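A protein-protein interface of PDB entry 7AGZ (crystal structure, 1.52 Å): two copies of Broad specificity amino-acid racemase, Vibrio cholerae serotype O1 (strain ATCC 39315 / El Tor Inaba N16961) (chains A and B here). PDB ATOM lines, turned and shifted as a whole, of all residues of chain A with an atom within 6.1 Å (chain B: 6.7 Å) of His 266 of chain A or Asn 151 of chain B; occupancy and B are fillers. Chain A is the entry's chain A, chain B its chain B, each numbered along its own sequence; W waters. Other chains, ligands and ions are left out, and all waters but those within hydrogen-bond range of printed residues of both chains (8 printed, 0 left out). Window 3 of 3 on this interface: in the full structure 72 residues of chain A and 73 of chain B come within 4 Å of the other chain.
Hydrophobic or aromatic side chains of chain A within 4 Å of the printed part of chain B: His 266 and Leu 268.
O of Ser 264 of chain A sits at hydrogen-bond distance from N of Asn 290 of chain A, 2.9 Å away.
ND2 of Asn 151 of chain B lies close to NE of Arg 150 of chain B, 3.5 Å away.
The backbone NH of Leu 288 of chain A lies within hydrogen-bond range of the backbone carbonyl oxygen of His 266 of chain A (2.8 Å).
NE2 of Gln 122 of chain B lies within hydrogen-bond range of OG of Ser 99 of chain B, at 3.3 Å.
The backbone carbonyl oxygen of Leu 268 of chain A sits at hydrogen-bond distance from the backbone NH of Ser 286 of chain A, at 2.9 Å.
The side-chain hydroxyl of Thr 119 of chain B sits at hydrogen-bond distance from the side-chain amide oxygen of Gln 122 of chain B.
Water W8 lies within hydrogen-bond range of the side-chain amide oxygen of Asn 290 of chain A, the side-chain hydroxyl of Thr 326 of chain A and the backbone carbonyl oxygen of Ser 99 of chain B.
Water W5 bridges the side-chain carboxylate (OE1) of Glu 163 of chain B (2.7 Å) and the backbone NH (N) of His 267 of chain A (2.9 Å).
Water W4 lies within hydrogen-bond range of O of Gly 118 of chain B, ND1 of His 266 of chain A and O of Gly 152 of chain B.
Water W2 lies within hydrogen-bond range of the side-chain hydroxyl (OG1) of Thr 326 of chain A (2.8 Å), the side-chain amide nitrogen (ND2) of Asn 151 of chain B (2.9 Å) and the guanidinium group (NE) of Arg 150 of chain B (3.2 Å).
Water W3 lies within hydrogen-bond range of the backbone carbonyl oxygen (O) of Leu 265 of chain A, the side-chain carboxylate (OE2) of Glu 163 of chain B and a ring nitrogen (ND1) of His 267 of chain A.
Water W1 bridges the side-chain hydroxyl (OG1) of Thr 119 of chain B (3.0 Å) and the backbone NH (N) of Leu 265 of chain A (3.0 Å).
No position is printed for both chains.
Of the 15 pairs that touch across the chains among the printed residues, none has its exchanged pair printed and touching as well.
The backbone carbonyl oxygen (O) of Arg 150 of chain B is in hydrogen-bond range of the side-chain amide nitrogen (ND2) of Asn 290 of chain A, 3.0 Å away.
The side-chain hydroxyl (OG) of Ser 264 of chain A is in hydrogen-bond range of the side-chain hydroxyl (OG) of Ser 99 of chain B (2.6 Å).
ND1 of His 266 of chain A is in hydrogen-bond range of O of Gly 152 of chain B (3.2 Å).
The side-chain amide nitrogen (ND2) of Asn 290 of chain A sits at hydrogen-bond distance from the side-chain amide oxygen (OD1) of Asn 151 of chain B (2.9 Å).
Of the printed residues of chain B, Leu 265 of chain A touches Thr 119.
Of the printed residues of chain B, His 266 of chain A touches Gly 118 (3.999 Å), Thr 119 (3.5 Å), Arg 150 (3.5 Å), Asn 151 (3.5 Å) and Gly 152 (3.2 Å).
Of the printed residues of chain A, Arg 98 of chain B touches Thr 326.
Of the printed residues of chain A, Ser 99 of chain B touches Ser 264 and Asn 290.
Printed residues of chain A within 4 Å of Gly 118 of chain B: His 266 (3.999 Å).
Of the printed residues of chain A, Asn 151 of chain B touches His 266 (3.5 Å) and Asn 290 (2.9 Å).
The nearest printed residue of chain B that does not touch His 266 of chain A is Gln 122 of chain B (4.4 Å).
The nearest printed residue of chain A that does not touch Asp 154 of chain B is His 267 of chain A (4.2 Å).
Gln 122 of chain B touches Ser 264 of chain A (CD to CB, 3.8 Å).
Thr 119 of chain B touches Leu 265 of chain A (CG2 to O, 3.2 Å).
ND1 of His 266 of chain A touches O of Gly 118 of chain B, 3.999 Å away.
CE1 of His 266 of chain A touches CG2 of Thr 119 of chain B (3.5 Å).
His 266 of chain A touches Arg 150 of chain B (CE1 to O, 3.5 Å).
CE1 of His 266 of chain A touches O of Asn 151 of chain B, at 3.5 Å.
Asn 144 of chain B touches Leu 268 of chain A (ND2 to CD1, 3.5 Å).
CD1 of Leu 268 of chain A touches CB of Asp 154 of chain B, at 3.8 Å.
OD1 of Asn 290 of chain A touches CB of Ser 99 of chain B, 3.5 Å away.
Thr 326 of chain A touches Arg 150 of chain B.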
ATOM      1  N   SER A 264      12.189  -5.390   5.385  1.00  0.00           N
ATOM      2  CA  SER A 264      11.264  -6.106   6.293  1.00  0.00           C
ATOM      3  C   SER A 264       9.963  -6.485   5.568  1.00  0.00           C
ATOM      4  O   SER A 264       9.680  -5.942   4.574  1.00  0.00           O
ATOM      5  CB  SER A 264      11.028  -5.279   7.539  1.00  0.00           C
ATOM      6  OG  SER A 264      10.888  -3.930   7.219  1.00  0.00           O
ATOM      7  N   LEU A 265       9.269  -7.455   6.144  1.00  0.00           N
ATOM      8  CA  LEU A 265       7.999  -7.998   5.592  1.00  0.00           C
ATOM      9  C   LEU A 265       6.926  -7.856   6.663  1.00  0.00           C
ATOM     10  O   LEU A 265       7.104  -8.385   7.709  1.00  0.00           O
ATOM     11  CB  LEU A 265       8.198  -9.473   5.267  1.00  0.00           C
ATOM     12  CG  LEU A 265       9.146  -9.720   4.109  1.00  0.00           C
ATOM     13  CD1 LEU A 265       9.372 -11.202   3.874  1.00  0.00           C
ATOM     14  CD2 LEU A 265       8.629  -9.079   2.833  1.00  0.00           C
ATOM     15  N   HIS A 266       5.868  -7.154   6.317  1.00  0.00           N
ATOM     16  CA  HIS A 266       4.837  -6.747   7.284  1.00  0.00           C
ATOM     17  C   HIS A 266       3.485  -7.346   6.907  1.00  0.00           C
ATOM     18  O   HIS A 266       3.074  -7.282   5.748  1.00  0.00           O
ATOM     19  CB  HIS A 266       4.735  -5.221   7.327  1.00  0.00           C
ATOM     20  CG  HIS A 266       6.016  -4.542   7.694  1.00  0.00           C
ATOM     21  ND1 HIS A 266       6.213  -3.905   8.909  1.00  0.00           N
ATOM     22  CD2 HIS A 266       7.161  -4.372   6.988  1.00  0.00           C
ATOM     23  CE1 HIS A 266       7.447  -3.434   8.943  1.00  0.00           C
ATOM     24  NE2 HIS A 266       8.024  -3.649   7.771  1.00  0.00           N
ATOM     25  N   HIS A 267       2.793  -7.948   7.874  1.00  0.00           N
ATOM     26  CA  HIS A 267       1.447  -8.468   7.638  1.00  0.00           C
ATOM     27  C   HIS A 267       0.454  -7.355   7.931  1.00  0.00           C
ATOM     28  O   HIS A 267       0.413  -6.843   9.060  1.00  0.00           O
ATOM     29  CB  HIS A 267       1.202  -9.693   8.525  1.00  0.00           C
ATOM     30  CG  HIS A 267       2.026 -10.881   8.139  1.00  0.00           C
ATOM     31  ND1 HIS A 267       3.400 -10.915   8.272  1.00  0.00           N
ATOM     32  CD2 HIS A 267       1.663 -12.094   7.654  1.00  0.00           C
ATOM     33  CE1 HIS A 267       3.850 -12.090   7.860  1.00  0.00           C
ATOM     34  NE2 HIS A 267       2.815 -12.827   7.496  1.00  0.00           N
ATOM     35  N   LEU A 268      -0.382  -7.024   6.947  1.00  0.00           N
ATOM     36  CA  LEU A 268      -1.366  -5.950   7.136  1.00  0.00           C
ATOM     37  C   LEU A 268      -2.742  -6.478   6.762  1.00  0.00           C
ATOM     38  O   LEU A 268      -2.915  -6.976   5.651  1.00  0.00           O
ATOM     39  CB  LEU A 268      -0.979  -4.749   6.246  1.00  0.00           C
ATOM     40  CG  LEU A 268      -1.536  -3.372   6.585  1.00  0.00           C
ATOM     41  CD1 LEU A 268      -1.080  -2.944   7.979  1.00  0.00           C
ATOM     42  CD2 LEU A 268      -1.149  -2.320   5.566  1.00  0.00           C
ATOM     43  N   SER A 286      -2.744  -8.977   3.522  1.00  0.00           N
ATOM     44  CA  SER A 286      -1.580  -8.726   2.691  1.00  0.00           C
ATOM     45  C   SER A 286      -0.259  -8.989   3.390  1.00  0.00           C
ATOM     46  O   SER A 286      -0.160  -8.988   4.616  1.00  0.00           O
ATOM     47  CB  SER A 286      -1.568  -7.237   2.243  1.00  0.00           C
ATOM     48  OG  SER A 286      -2.748  -6.975   1.504  1.00  0.00           O
ATOM     49  N   VAL A 287       0.780  -9.225   2.600  1.00  0.00           N
ATOM     50  CA  VAL A 287       2.156  -9.158   3.093  1.00  0.00           C
ATOM     51  C   VAL A 287       2.835  -8.072   2.278  1.00  0.00           C
ATOM     52  O   VAL A 287       2.887  -8.156   1.041  1.00  0.00           O
ATOM     53  CB  VAL A 287       2.900 -10.509   2.983  1.00  0.00           C
ATOM     54  CG1 VAL A 287       4.309 -10.349   3.550  1.00  0.00           C
ATOM     55  CG2 VAL A 287       2.158 -11.618   3.732  1.00  0.00           C
ATOM     56  N   LEU A 288       3.336  -7.048   2.958  1.00  0.00           N
ATOM     57  CA  LEU A 288       3.995  -5.914   2.313  1.00  0.00           C
ATOM     58  C   LEU A 288       5.506  -5.929   2.568  1.00  0.00           C
ATOM     59  O   LEU A 288       5.964  -6.126   3.694  1.00  0.00           O
ATOM     60  CB  LEU A 288       3.373  -4.606   2.785  1.00  0.00           C
ATOM     61  CG  LEU A 288       1.848  -4.536   2.556  1.00  0.00           C
ATOM     62  CD1 LEU A 288       1.357  -3.148   3.026  1.00  0.00           C
ATOM     63  CD2 LEU A 288       1.396  -4.756   1.135  1.00  0.00           C
ATOM     64  N   ALA A 289       6.280  -5.707   1.519  1.00  0.00           N
ATOM     65  CA  ALA A 289       7.736  -5.533   1.617  1.00  0.00           C
ATOM     66  C   ALA A 289       8.092  -4.066   1.764  1.00  0.00           C
ATOM     67  O   ALA A 289       7.631  -3.234   0.985  1.00  0.00           O
ATOM     68  CB  ALA A 289       8.442  -6.128   0.397  1.00  0.00           C
ATOM     69  N   ASN A 290       8.876  -3.769   2.792  1.00  0.00           N
ATOM     70  CA  ASN A 290       9.346  -2.422   3.123  1.00  0.00           C
ATOM     71  C   ASN A 290      10.741  -2.274   2.536  1.00  0.00           C
ATOM     72  O   ASN A 290      11.641  -3.052   2.886  1.00  0.00           O
ATOM     73  CB  ASN A 290       9.315  -2.279   4.646  1.00  0.00           C
ATOM     74  CG  ASN A 290       9.808  -0.914   5.156  1.00  0.00           C
ATOM     75  OD1 ASN A 290      10.817  -0.360   4.700  1.00  0.00           O
ATOM     76  ND2 ASN A 290       9.054  -0.346   6.139  1.00  0.00           N
ATOM     77  N   THR A 326      11.447   5.605   2.051  1.00  0.00           N
ATOM     78  CA  THR A 326      10.878   4.255   2.118  1.00  0.00           C
ATOM     79  C   THR A 326       9.788   4.048   1.081  1.00  0.00           C
ATOM     80  O   THR A 326       9.023   4.964   0.776  1.00  0.00           O
ATOM     81  CB  THR A 326      10.333   4.005   3.545  1.00  0.00           C
ATOM     82  OG1 THR A 326      11.393   4.082   4.501  1.00  0.00           O
ATOM     83  CG2 THR A 326       9.635   2.645   3.678  1.00  0.00           C
ATOM     84  N   VAL B  97      14.748   6.505  11.586  1.00  0.00           N
ATOM     85  CA  VAL B  97      13.317   6.721  11.414  1.00  0.00           C
ATOM     86  C   VAL B  97      12.708   5.840  10.344  1.00  0.00           C
ATOM     87  O   VAL B  97      11.581   6.115   9.889  1.00  0.00           O
ATOM     88  CB  VAL B  97      12.965   8.204  11.217  1.00  0.00           C
ATOM     89  CG1 VAL B  97      13.389   8.988  12.475  1.00  0.00           C
ATOM     90  CG2 VAL B  97      13.660   8.742  10.001  1.00  0.00           C
ATOM     91  N   ARG B  98      13.425   4.798   9.896  1.00  0.00           N
ATOM     92  CA  ARG B  98      12.847   3.861   8.951  1.00  0.00           C
ATOM     93  C   ARG B  98      13.369   2.480   9.269  1.00  0.00           C
ATOM     94  O   ARG B  98      14.394   2.339   9.923  1.00  0.00           O
ATOM     95  CB  ARG B  98      13.197   4.253   7.504  1.00  0.00           C
ATOM     96  CG  ARG B  98      14.720   4.312   7.169  1.00  0.00           C
ATOM     97  CD  ARG B  98      15.003   4.096   5.647  1.00  0.00           C
ATOM     98  NE  ARG B  98      16.385   4.326   5.212  1.00  0.00           N
ATOM     99  CZ  ARG B  98      17.393   3.470   5.346  1.00  0.00           C
ATOM    100  NH1 ARG B  98      17.206   2.286   5.980  1.00  0.00           N
ATOM    101  NH2 ARG B  98      18.604   3.781   4.844  1.00  0.00           N
ATOM    102  N   SER B  99      12.643   1.480   8.781  1.00  0.00           N
ATOM    103  CA  SER B  99      13.143   0.111   8.649  1.00  0.00           C
ATOM    104  C   SER B  99      14.481   0.110   7.897  1.00  0.00           C
ATOM    105  O   SER B  99      14.689   0.874   6.934  1.00  0.00           O
ATOM    106  CB  SER B  99      12.090  -0.702   7.908  1.00  0.00           C
ATOM    107  OG  SER B  99      12.549  -2.044   7.761  1.00  0.00           O
ATOM    108  N   ALA B 100      15.444  -0.690   8.375  1.00  0.00           N
ATOM    109  CA  ALA B 100      16.742  -0.794   7.720  1.00  0.00           C
ATOM    110  C   ALA B 100      17.140  -2.248   7.602  1.00  0.00           C
ATOM    111  O   ALA B 100      16.836  -3.047   8.489  1.00  0.00           O
ATOM    112  CB  ALA B 100      17.800  -0.010   8.524  1.00  0.00           C
ATOM    113  N   LEU B 116      14.433   1.015  14.552  1.00  0.00           N
ATOM    114  CA  LEU B 116      12.972   1.118  14.523  1.00  0.00           C
ATOM    115  C   LEU B 116      12.415  -0.171  13.945  1.00  0.00           C
ATOM    116  O   LEU B 116      12.609  -0.444  12.748  1.00  0.00           O
ATOM    117  CB  LEU B 116      12.533   2.284  13.639  1.00  0.00           C
ATOM    118  CG  LEU B 116      11.020   2.559  13.564  1.00  0.00           C
ATOM    119  CD1 LEU B 116      10.536   2.984  14.961  1.00  0.00           C
ATOM    120  CD2 LEU B 116      10.693   3.657  12.527  1.00  0.00           C
ATOM    121  N   ILE B 117      11.756  -0.972  14.772  1.00  0.00           N
ATOM    122  CA  ILE B 117      11.335  -2.307  14.339  1.00  0.00           C
ATOM    123  C   ILE B 117       9.835  -2.484  14.469  1.00  0.00           C
ATOM    124  O   ILE B 117       9.196  -1.918  15.369  1.00  0.00           O
ATOM    125  CB  ILE B 117      12.084  -3.388  15.117  1.00  0.00           C
ATOM    126  CG1 ILE B 117      11.728  -3.371  16.604  1.00  0.00           C
ATOM    127  CG2 ILE B 117      13.608  -3.255  14.879  1.00  0.00           C
ATOM    128  CD1 ILE B 117      12.494  -4.475  17.388  1.00  0.00           C
ATOM    129  N   GLY B 118       9.274  -3.258  13.517  1.00  0.00           N
ATOM    130  CA  GLY B 118       7.849  -3.514  13.416  1.00  0.00           C
ATOM    131  C   GLY B 118       7.507  -4.948  13.043  1.00  0.00           C
ATOM    132  O   GLY B 118       6.347  -5.205  12.688  1.00  0.00           O
ATOM    133  N   THR B 119       8.481  -5.857  13.073  1.00  0.00           N
ATOM    134  CA  THR B 119       8.264  -7.264  12.720  1.00  0.00           C
ATOM    135  C   THR B 119       9.086  -8.181  13.607  1.00  0.00           C
ATOM    136  O   THR B 119      10.156  -7.813  14.094  1.00  0.00           O
ATOM    137  CB  THR B 119       8.679  -7.579  11.251  1.00  0.00           C
ATOM    138  OG1 THR B 119      10.108  -7.477  11.170  1.00  0.00           O
ATOM    139  CG2 THR B 119       8.049  -6.616  10.240  1.00  0.00           C
ATOM    140  N   GLN B 122      12.716  -8.682  12.429  1.00  0.00           N
ATOM    141  CA  GLN B 122      13.648  -7.628  12.800  1.00  0.00           C
ATOM    142  C   GLN B 122      14.097  -7.803  14.241  1.00  0.00           C
ATOM    143  O   GLN B 122      15.278  -7.622  14.564  1.00  0.00           O
ATOM    144  CB  GLN B 122      13.029  -6.225  12.663  1.00  0.00           C
ATOM    145  CG  GLN B 122      12.930  -5.727  11.240  1.00  0.00           C
ATOM    146  CD  GLN B 122      11.965  -4.588  11.155  1.00  0.00           C
ATOM    147  OE1 GLN B 122      10.778  -4.763  11.456  1.00  0.00           O
ATOM    148  NE2 GLN B 122      12.429  -3.435  10.730  1.00  0.00           N
ATOM    149  N   ILE B 141       9.740   0.409  19.123  1.00  0.00           N
ATOM    150  CA  ILE B 141       8.721  -0.425  18.466  1.00  0.00           C
ATOM    151  C   ILE B 141       7.746   0.474  17.746  1.00  0.00           C
ATOM    152  O   ILE B 141       7.117   1.355  18.352  1.00  0.00           O
ATOM    153  CB  ILE B 141       7.981  -1.337  19.445  1.00  0.00           C
ATOM    154  CG1 ILE B 141       9.002  -2.194  20.196  1.00  0.00           C
ATOM    155  CG2 ILE B 141       6.995  -2.183  18.691  1.00  0.00           C
ATOM    156  CD1 ILE B 141       8.409  -3.108  21.222  1.00  0.00           C
ATOM    157  N   ALA B 142       7.624   0.268  16.454  1.00  0.00           N
ATOM    158  CA  ALA B 142       6.670   1.005  15.651  1.00  0.00           C
ATOM    159  C   ALA B 142       5.336   0.289  15.643  1.00  0.00           C
ATOM    160  O   ALA B 142       5.257  -0.864  15.193  1.00  0.00           O
ATOM    161  CB  ALA B 142       7.198   1.157  14.223  1.00  0.00           C
ATOM    162  N   LEU B 143       4.263   0.975  16.055  1.00  0.00           N
ATOM    163  CA  LEU B 143       2.903   0.463  16.030  1.00  0.00           C
ATOM    164  C   LEU B 143       2.146   1.125  14.888  1.00  0.00           C
ATOM    165  O   LEU B 143       2.481   2.232  14.472  1.00  0.00           O
ATOM    166  CB  LEU B 143       2.176   0.744  17.347  1.00  0.00           C
ATOM    167  CG  LEU B 143       2.764   0.260  18.671  1.00  0.00           C
ATOM    168  CD1 LEU B 143       1.765   0.434  19.817  1.00  0.00           C
ATOM    169  CD2 LEU B 143       3.258  -1.167  18.608  1.00  0.00           C
ATOM    170  N   ASN B 144       1.148   0.430  14.346  1.00  0.00           N
ATOM    171  CA  ASN B 144       0.384   0.928  13.208  1.00  0.00           C
ATOM    172  C   ASN B 144      -0.917   1.665  13.562  1.00  0.00           C
ATOM    173  O   ASN B 144      -1.779   1.787  12.707  1.00  0.00           O
ATOM    174  CB  ASN B 144       0.114  -0.215  12.219  1.00  0.00           C
ATOM    175  CG  ASN B 144      -0.233   0.309  10.801  1.00  0.00           C
ATOM    176  OD1 ASN B 144       0.406   1.221  10.284  1.00  0.00           O
ATOM    177  ND2 ASN B 144      -1.305  -0.254  10.204  1.00  0.00           N
ATOM    178  N   MET B 148      -0.137   4.282   8.845  1.00  0.00           N
ATOM    179  CA  MET B 148       0.832   4.446   7.761  1.00  0.00           C
ATOM    180  C   MET B 148       1.049   3.148   6.993  1.00  0.00           C
ATOM    181  O   MET B 148       1.395   3.196   5.810  1.00  0.00           O
ATOM    182  CB  MET B 148       2.186   4.934   8.293  1.00  0.00           C
ATOM    183  CG  MET B 148       2.279   6.395   8.626  1.00  0.00           C
ATOM    184  SD  MET B 148       2.154   7.373   7.069  1.00  0.00           S
ATOM    185  CE  MET B 148       3.722   7.186   6.214  1.00  0.00           C
ATOM    186  N   GLY B 149       0.833   1.997   7.628  1.00  0.00           N
ATOM    187  CA  GLY B 149       1.089   0.723   6.942  1.00  0.00           C
ATOM    188  C   GLY B 149       2.492   0.604   6.398  1.00  0.00           C
ATOM    189  O   GLY B 149       2.682   0.046   5.313  1.00  0.00           O
ATOM    190  N   ARG B 150       3.504   1.045   7.174  1.00  0.00           N
ATOM    191  CA  ARG B 150       4.860   1.250   6.648  1.00  0.00           C
ATOM    192  C   ARG B 150       5.881   0.505   7.512  1.00  0.00           C
ATOM    193  O   ARG B 150       6.230  -0.658   7.232  1.00  0.00           O
ATOM    194  CB  ARG B 150       5.152   2.758   6.542  1.00  0.00           C
ATOM    195  CG  ARG B 150       6.437   3.046   5.846  1.00  0.00           C
ATOM    196  CD  ARG B 150       6.595   4.546   5.611  1.00  0.00           C
ATOM    197  NE  ARG B 150       6.752   5.263   6.870  1.00  0.00           N
ATOM    198  CZ  ARG B 150       7.192   6.515   6.949  1.00  0.00           C
ATOM    199  NH1 ARG B 150       7.464   7.223   5.829  1.00  0.00           N
ATOM    200  NH2 ARG B 150       7.373   7.097   8.142  1.00  0.00           N
ATOM    201  N   ASN B 151       6.369   1.153   8.584  1.00  0.00           N
ATOM    202  CA  ASN B 151       7.390   0.498   9.392  1.00  0.00           C
ATOM    203  C   ASN B 151       6.854  -0.285  10.596  1.00  0.00           C
ATOM    204  O   ASN B 151       7.658  -0.897  11.295  1.00  0.00           O
ATOM    205  CB  ASN B 151       8.362   1.570   9.937  1.00  0.00           C
ATOM    206  CG  ASN B 151       9.121   2.316   8.839  1.00  0.00           C
ATOM    207  OD1 ASN B 151       9.817   1.697   7.997  1.00  0.00           O
ATOM    208  ND2 ASN B 151       9.058   3.629   8.849  1.00  0.00           N
ATOM    209  N   GLY B 152       5.545  -0.204  10.899  1.00  0.00           N
ATOM    210  CA  GLY B 152       5.004  -0.667  12.146  1.00  0.00           C
ATOM    211  C   GLY B 152       4.361  -2.037  12.135  1.00  0.00           C
ATOM    212  O   GLY B 152       4.194  -2.682  11.090  1.00  0.00           O
ATOM    213  N   ILE B 153       4.007  -2.492  13.345  1.00  0.00           N
ATOM    214  CA  ILE B 153       3.209  -3.720  13.532  1.00  0.00           C
ATOM    215  C   ILE B 153       1.751  -3.370  13.714  1.00  0.00           C
ATOM    216  O   ILE B 153       1.378  -2.647  14.647  1.00  0.00           O
ATOM    217  CB  ILE B 153       3.731  -4.574  14.704  1.00  0.00           C
ATOM    218  CG1 ILE B 153       2.902  -5.846  14.922  1.00  0.00           C
ATOM    219  CG2 ILE B 153       3.803  -3.845  16.024  1.00  0.00           C
ATOM    220  CD1 ILE B 153       2.975  -6.827  13.728  1.00  0.00           C
ATOM    221  N   ASP B 154       0.912  -3.904  12.842  1.00  0.00           N
ATOM    222  CA  ASP B 154      -0.521  -3.742  12.982  1.00  0.00           C
ATOM    223  C   ASP B 154      -1.052  -4.705  14.043  1.00  0.00           C
ATOM    224  O   ASP B 154      -0.743  -5.916  14.018  1.00  0.00           O
ATOM    225  CB  ASP B 154      -1.244  -3.957  11.653  1.00  0.00           C
ATOM    226  CG  ASP B 154      -2.695  -3.582  11.771  1.00  0.00           C
ATOM    227  OD1 ASP B 154      -3.514  -4.427  12.189  1.00  0.00           O
ATOM    228  OD2 ASP B 154      -2.988  -2.394  11.478  1.00  0.00           O
ATOM    229  N   GLU B 163       2.234 -10.968  17.608  1.00  0.00           N
ATOM    230  CA  GLU B 163       3.532 -10.599  17.058  1.00  0.00           C
ATOM    231  C   GLU B 163       4.114  -9.394  17.798  1.00  0.00           C
ATOM    232  O   GLU B 163       5.317  -9.364  18.074  1.00  0.00           O
ATOM    233  CB  GLU B 163       3.435 -10.330  15.537  1.00  0.00           C
ATOM    234  CG  GLU B 163       4.805 -10.003  14.898  1.00  0.00           C
ATOM    235  CD  GLU B 163       4.810  -9.935  13.358  1.00  0.00           C
ATOM    236  OE1 GLU B 163       3.711 -10.035  12.744  1.00  0.00           O
ATOM    237  OE2 GLU B 163       5.923  -9.753  12.754  1.00  0.00           O
ATOM    238  N   MET B 179       6.164   3.932  19.359  1.00  0.00           N
ATOM    239  CA  MET B 179       5.845   5.098  18.522  1.00  0.00           C
ATOM    240  C   MET B 179       4.777   4.732  17.507  1.00  0.00           C
ATOM    241  O   MET B 179       4.555   3.564  17.227  1.00  0.00           O
ATOM    242  CB  MET B 179       7.094   5.643  17.835  1.00  0.00           C
ATOM    243  CG  MET B 179       7.718   4.671  16.836  1.00  0.00           C
ATOM    244  SD  MET B 179       6.955   4.627  15.204  1.00  0.00           S
ATOM    245  CE  MET B 179       7.662   6.065  14.401  1.00  0.00           C
HETATM  246  O   HOH W   1      10.731  -8.580   8.495  1.00  0.00           O
HETATM  247  O   HOH W   2       9.933   5.206   6.634  1.00  0.00           O
HETATM  248  O   HOH W   3       6.240 -10.124   9.824  1.00  0.00           O
HETATM  249  O   HOH W   4       4.528  -5.868  10.687  1.00  0.00           O
HETATM  250  O   HOH W   5       3.832  -8.464  10.543  1.00  0.00           O
HETATM  251  O   HOH W   6       1.981  -4.817  10.228  1.00  0.00           O
HETATM  252  O   HOH W   7      -0.334  -7.697  11.829  1.00  0.00           O
HETATM  253  O   HOH W   8      12.505   1.601   5.023  1.00  0.00           O
